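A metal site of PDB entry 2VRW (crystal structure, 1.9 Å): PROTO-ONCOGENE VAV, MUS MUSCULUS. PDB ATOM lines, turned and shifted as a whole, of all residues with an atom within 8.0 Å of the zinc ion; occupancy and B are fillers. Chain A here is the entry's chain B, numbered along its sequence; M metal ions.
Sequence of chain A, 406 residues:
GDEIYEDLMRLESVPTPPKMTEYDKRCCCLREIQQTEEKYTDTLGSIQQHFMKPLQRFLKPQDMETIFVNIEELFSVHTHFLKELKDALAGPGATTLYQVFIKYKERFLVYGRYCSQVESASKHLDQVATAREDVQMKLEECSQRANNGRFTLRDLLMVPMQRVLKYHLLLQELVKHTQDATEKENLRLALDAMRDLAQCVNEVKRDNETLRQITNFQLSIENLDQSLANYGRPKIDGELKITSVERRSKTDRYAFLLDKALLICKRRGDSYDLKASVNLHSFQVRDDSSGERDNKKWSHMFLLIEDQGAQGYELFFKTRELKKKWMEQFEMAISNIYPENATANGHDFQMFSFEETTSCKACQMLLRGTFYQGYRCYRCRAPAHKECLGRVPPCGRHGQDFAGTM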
ATOM      1  N   ALA A 342     -17.414  26.202 -23.483  1.00  0.00           N
ATOM      2  CA  ALA A 342     -18.455  25.176 -23.431  1.00  0.00           C
ATOM      3  C   ALA A 342     -17.888  23.779 -23.187  1.00  0.00           C
ATOM      4  O   ALA A 342     -18.517  22.954 -22.554  1.00  0.00           O
ATOM      5  CB  ALA A 342     -19.288  25.201 -24.711  1.00  0.00           C
ATOM      6  N   ALA A 344     -14.598  23.397 -21.937  1.00  0.00           N
ATOM      7  CA  ALA A 344     -13.429  23.575 -21.087  1.00  0.00           C
ATOM      8  C   ALA A 344     -13.354  22.481 -20.032  1.00  0.00           C
ATOM      9  O   ALA A 344     -14.376  22.039 -19.500  1.00  0.00           O
ATOM     10  CB  ALA A 344     -13.457  24.950 -20.422  1.00  0.00           C
ATOM     11  N   ASN A 345     -12.123  22.027 -19.746  1.00  0.00           N
ATOM     12  CA  ASN A 345     -11.865  21.169 -18.592  1.00  0.00           C
ATOM     13  C   ASN A 345     -12.667  19.866 -18.578  1.00  0.00           C
ATOM     14  O   ASN A 345     -13.024  19.342 -17.525  1.00  0.00           O
ATOM     15  CB  ASN A 345     -12.060  21.954 -17.282  1.00  0.00           C
ATOM     16  CG  ASN A 345     -11.195  23.207 -17.214  1.00  0.00           C
ATOM     17  OD1 ASN A 345     -11.676  24.315 -16.956  1.00  0.00           O
ATOM     18  ND2 ASN A 345      -9.894  23.033 -17.455  1.00  0.00           N
ATOM     19  N   GLY A 346     -12.929  19.348 -19.773  1.00  0.00           N
ATOM     20  CA  GLY A 346     -13.590  18.057 -19.931  1.00  0.00           C
ATOM     21  C   GLY A 346     -15.106  18.093 -19.990  1.00  0.00           C
ATOM     22  O   GLY A 346     -15.742  17.068 -20.272  1.00  0.00           O
ATOM     23  N   HIS A 347     -15.692  19.263 -19.732  1.00  0.00           N
ATOM     24  CA  HIS A 347     -17.143  19.414 -19.706  1.00  0.00           C
ATOM     25  C   HIS A 347     -17.760  19.433 -21.126  1.00  0.00           C
ATOM     26  O   HIS A 347     -17.051  19.480 -22.137  1.00  0.00           O
ATOM     27  CB  HIS A 347     -17.550  20.697 -18.963  1.00  0.00           C
ATOM     28  CG  HIS A 347     -17.116  20.749 -17.524  1.00  0.00           C
ATOM     29  ND1 HIS A 347     -17.719  19.991 -16.541  1.00  0.00           N
ATOM     30  CD2 HIS A 347     -16.195  21.514 -16.898  1.00  0.00           C
ATOM     31  CE1 HIS A 347     -17.144  20.251 -15.378  1.00  0.00           C
ATOM     32  NE2 HIS A 347     -16.215  21.172 -15.570  1.00  0.00           N
ATOM     33  N   ASP A 348     -19.096  19.380 -21.169  1.00  0.00           N
ATOM     34  CA  ASP A 348     -19.870  19.623 -22.391  1.00  0.00           C
ATOM     35  C   ASP A 348     -21.150  20.400 -22.007  1.00  0.00           C
ATOM     36  O   ASP A 348     -22.222  19.822 -21.838  1.00  0.00           O
ATOM     37  CB  ASP A 348     -20.212  18.303 -23.083  1.00  0.00           C
ATOM     38  CG  ASP A 348     -20.871  18.484 -24.450  1.00  0.00           C
ATOM     39  OD1 ASP A 348     -21.238  19.617 -24.840  1.00  0.00           O
ATOM     40  OD2 ASP A 348     -21.036  17.452 -25.141  1.00  0.00           O
ATOM     41  N   PHE A 349     -20.994  21.706 -21.853  1.00  0.00           N
ATOM     42  CA  PHE A 349     -22.072  22.566 -21.355  1.00  0.00           C
ATOM     43  C   PHE A 349     -23.069  22.860 -22.460  1.00  0.00           C
ATOM     44  O   PHE A 349     -22.681  23.191 -23.583  1.00  0.00           O
ATOM     45  CB  PHE A 349     -21.513  23.884 -20.812  1.00  0.00           C
ATOM     46  CG  PHE A 349     -20.804  23.744 -19.511  1.00  0.00           C
ATOM     47  CD1 PHE A 349     -21.506  23.468 -18.333  1.00  0.00           C
ATOM     48  CD2 PHE A 349     -19.421  23.883 -19.445  1.00  0.00           C
ATOM     49  CE1 PHE A 349     -20.838  23.332 -17.122  1.00  0.00           C
ATOM     50  CE2 PHE A 349     -18.744  23.757 -18.240  1.00  0.00           C
ATOM     51  CZ  PHE A 349     -19.462  23.470 -17.068  1.00  0.00           C
ATOM     52  N   ARG A 376     -25.888  23.450 -18.310  1.00  0.00           N
ATOM     53  CA  ARG A 376     -25.720  22.223 -17.536  1.00  0.00           C
ATOM     54  C   ARG A 376     -24.774  21.311 -18.306  1.00  0.00           C
ATOM     55  O   ARG A 376     -24.965  21.089 -19.506  1.00  0.00           O
ATOM     56  CB  ARG A 376     -27.079  21.542 -17.342  1.00  0.00           C
ATOM     57  CG  ARG A 376     -27.055  20.320 -16.444  1.00  0.00           C
ATOM     58  CD  ARG A 376     -28.233  19.433 -16.806  1.00  0.00           C
ATOM     59  NE  ARG A 376     -28.789  18.729 -15.658  1.00  0.00           N
ATOM     60  CZ  ARG A 376     -29.756  17.807 -15.739  1.00  0.00           C
ATOM     61  NH1 ARG A 376     -30.251  17.456 -16.917  1.00  0.00           N
ATOM     62  NH2 ARG A 376     -30.208  17.223 -14.635  1.00  0.00           N
ATOM     63  N   CYS A 377     -23.752  20.793 -17.634  1.00  0.00           N
ATOM     64  CA  CYS A 377     -22.806  19.891 -18.298  1.00  0.00           C
ATOM     65  C   CYS A 377     -23.482  18.580 -18.601  1.00  0.00           C
ATOM     66  O   CYS A 377     -24.051  17.957 -17.706  1.00  0.00           O
ATOM     67  CB  CYS A 377     -21.554  19.649 -17.458  1.00  0.00           C
ATOM     68  SG  CYS A 377     -20.432  18.467 -18.279  1.00  0.00           S
ATOM     69  N   TYR A 378     -23.442  18.167 -19.864  1.00  0.00           N
ATOM     70  CA  TYR A 378     -24.044  16.915 -20.289  1.00  0.00           C
ATOM     71  C   TYR A 378     -23.442  15.716 -19.530  1.00  0.00           C
ATOM     72  O   TYR A 378     -24.161  14.787 -19.157  1.00  0.00           O
ATOM     73  CB  TYR A 378     -23.896  16.726 -21.801  1.00  0.00           C
ATOM     74  CG  TYR A 378     -24.435  15.401 -22.289  1.00  0.00           C
ATOM     75  CD1 TYR A 378     -25.809  15.178 -22.396  1.00  0.00           C
ATOM     76  CD2 TYR A 378     -23.562  14.380 -22.650  1.00  0.00           C
ATOM     77  CE1 TYR A 378     -26.304  13.967 -22.835  1.00  0.00           C
ATOM     78  CE2 TYR A 378     -24.051  13.162 -23.092  1.00  0.00           C
ATOM     79  CZ  TYR A 378     -25.421  12.964 -23.186  1.00  0.00           C
ATOM     80  OH  TYR A 378     -25.908  11.758 -23.623  1.00  0.00           O
ATOM     81  N   ARG A 379     -22.132  15.767 -19.302  1.00  0.00           N
ATOM     82  CA  ARG A 379     -21.415  14.658 -18.657  1.00  0.00           C
ATOM     83  C   ARG A 379     -21.672  14.537 -17.150  1.00  0.00           C
ATOM     84  O   ARG A 379     -22.109  13.488 -16.677  1.00  0.00           O
ATOM     85  CB  ARG A 379     -19.899  14.789 -18.896  1.00  0.00           C
ATOM     86  CG  ARG A 379     -19.438  14.608 -20.320  1.00  0.00           C
ATOM     87  CD  ARG A 379     -17.904  14.632 -20.399  1.00  0.00           C
ATOM     88  NE  ARG A 379     -17.278  13.440 -19.802  1.00  0.00           N
ATOM     89  CZ  ARG A 379     -16.001  13.366 -19.414  1.00  0.00           C
ATOM     90  NH1 ARG A 379     -15.192  14.408 -19.545  1.00  0.00           N
ATOM     91  NH2 ARG A 379     -15.528  12.243 -18.898  1.00  0.00           N
ATOM     92  N   CYS A 380     -21.401  15.610 -16.407  1.00  0.00           N
ATOM     93  CA  CYS A 380     -21.411  15.561 -14.933  1.00  0.00           C
ATOM     94  C   CYS A 380     -22.614  16.267 -14.287  1.00  0.00           C
ATOM     95  O   CYS A 380     -22.777  16.215 -13.052  1.00  0.00           O
ATOM     96  CB  CYS A 380     -20.116  16.181 -14.391  1.00  0.00           C
ATOM     97  SG  CYS A 380     -20.004  17.979 -14.646  1.00  0.00           S
ATOM     98  N   ARG A 381     -23.437  16.909 -15.116  1.00  0.00           N
ATOM     99  CA  ARG A 381     -24.657  17.612 -14.696  1.00  0.00           C
ATOM    100  C   ARG A 381     -24.406  18.903 -13.892  1.00  0.00           C
ATOM    101  O   ARG A 381     -25.322  19.459 -13.295  1.00  0.00           O
ATOM    102  CB  ARG A 381     -25.638  16.690 -13.951  1.00  0.00           C
ATOM    103  CG  ARG A 381     -26.053  15.401 -14.701  1.00  0.00           C
ATOM    104  CD  ARG A 381     -27.076  15.663 -15.813  1.00  0.00           C
ATOM    105  NE  ARG A 381     -27.704  14.424 -16.289  1.00  0.00           N
ATOM    106  CZ  ARG A 381     -27.538  13.893 -17.510  1.00  0.00           C
ATOM    107  NH1 ARG A 381     -26.773  14.492 -18.411  1.00  0.00           N
ATOM    108  NH2 ARG A 381     -28.159  12.768 -17.817  1.00  0.00           N
ATOM    109  N   ALA A 382     -23.157  19.394 -13.887  1.00  0.00           N
ATOM    110  CA  ALA A 382     -22.861  20.640 -13.180  1.00  0.00           C
ATOM    111  C   ALA A 382     -23.602  21.824 -13.823  1.00  0.00           C
ATOM    112  O   ALA A 382     -23.512  22.013 -15.042  1.00  0.00           O
ATOM    113  CB  ALA A 382     -21.353  20.897 -13.145  1.00  0.00           C
ATOM    114  N   PRO A 383     -24.359  22.611 -13.031  1.00  0.00           N
ATOM    115  CA  PRO A 383     -24.967  23.846 -13.527  1.00  0.00           C
ATOM    116  C   PRO A 383     -23.986  25.009 -13.471  1.00  0.00           C
ATOM    117  O   PRO A 383     -23.132  25.040 -12.576  1.00  0.00           O
ATOM    118  CB  PRO A 383     -26.124  24.111 -12.557  1.00  0.00           C
ATOM    119  CG  PRO A 383     -25.930  23.157 -11.400  1.00  0.00           C
ATOM    120  CD  PRO A 383     -24.683  22.363 -11.616  1.00  0.00           C
ATOM    121  N   VAL A 392     -15.644  26.362 -13.675  1.00  0.00           N
ATOM    122  CA  VAL A 392     -16.164  25.153 -13.053  1.00  0.00           C
ATOM    123  C   VAL A 392     -15.019  24.130 -12.932  1.00  0.00           C
ATOM    124  O   VAL A 392     -14.309  23.888 -13.906  1.00  0.00           O
ATOM    125  CB  VAL A 392     -17.358  24.557 -13.876  1.00  0.00           C
ATOM    126  CG1 VAL A 392     -17.933  23.313 -13.187  1.00  0.00           C
ATOM    127  CG2 VAL A 392     -18.447  25.609 -14.056  1.00  0.00           C
ATOM    128  N   PRO A 393     -14.816  23.541 -11.740  1.00  0.00           N
ATOM    129  CA  PRO A 393     -13.774  22.514 -11.551  1.00  0.00           C
ATOM    130  C   PRO A 393     -13.891  21.380 -12.591  1.00  0.00           C
ATOM    131  O   PRO A 393     -15.001  21.062 -13.024  1.00  0.00           O
ATOM    132  CB  PRO A 393     -14.050  21.992 -10.144  1.00  0.00           C
ATOM    133  CG  PRO A 393     -14.681  23.156  -9.435  1.00  0.00           C
ATOM    134  CD  PRO A 393     -15.541  23.817 -10.481  1.00  0.00           C
ATOM    135  N   PRO A 394     -12.751  20.767 -12.995  1.00  0.00           N
ATOM    136  CA  PRO A 394     -12.720  19.809 -14.092  1.00  0.00           C
ATOM    137  C   PRO A 394     -13.784  18.733 -14.000  1.00  0.00           C
ATOM    138  O   PRO A 394     -14.137  18.288 -12.897  1.00  0.00           O
ATOM    139  CB  PRO A 394     -11.318  19.190 -13.984  1.00  0.00           C
ATOM    140  CG  PRO A 394     -10.513  20.280 -13.420  1.00  0.00           C
ATOM    141  CD  PRO A 394     -11.397  20.954 -12.416  1.00  0.00           C
ATOM    142  N   CYS A 395     -14.290  18.310 -15.159  1.00  0.00           N
ATOM    143  CA  CYS A 395     -15.402  17.371 -15.260  1.00  0.00           C
ATOM    144  C   CYS A 395     -15.077  16.025 -14.610  1.00  0.00           C
ATOM    145  O   CYS A 395     -14.069  15.399 -14.920  1.00  0.00           O
ATOM    146  CB  CYS A 395     -15.783  17.183 -16.729  1.00  0.00           C
ATOM    147  SG  CYS A 395     -17.353  16.367 -17.000  1.00  0.00           S
HETATM  148 ZN    ZN M   1     -18.863  18.233 -16.625  1.00  0.00          ZN
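The zinc ion is bound by ND1 of His 347 (2.1 Å), SG of Cys 377 (2.3 Å), SG of Cys 380 (2.3 Å) and SG of Cys 395 (2.4 Å).
A ring nitrogen (NE2) of His 347 lies within hydrogen-bond range of the backbone carbonyl oxygen (O) of Pro 393 (2.8 Å). SG of Cys 377 sits close to N of Arg 379, 3.4 Å away. N of Asp 348 lies close to SG of Cys 377 (3.3 Å). The backbone NH (N) of Cys 377 sits at hydrogen-bond distance from the backbone carbonyl oxygen (O) of Ala 382, at 2.9 Å. The backbone NH (N) of Ala 382 lies close to the side-chain sulfur (SG) of Cys 380. O of Gly 346 lies close to SG of Cys 395 (3.7 Å). The backbone NH (N) of Cys 395 lies within hydrogen-bond range of the backbone carbonyl oxygen (O) of Asn 345, 2.9 Å away.
Four residues have an atom within 4 Å of the zinc ion: His 347, Cys 377, Cys 380 and Cys 395. Along chain A the residues within 4 Å of the zinc ion span positions 347 to 395.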
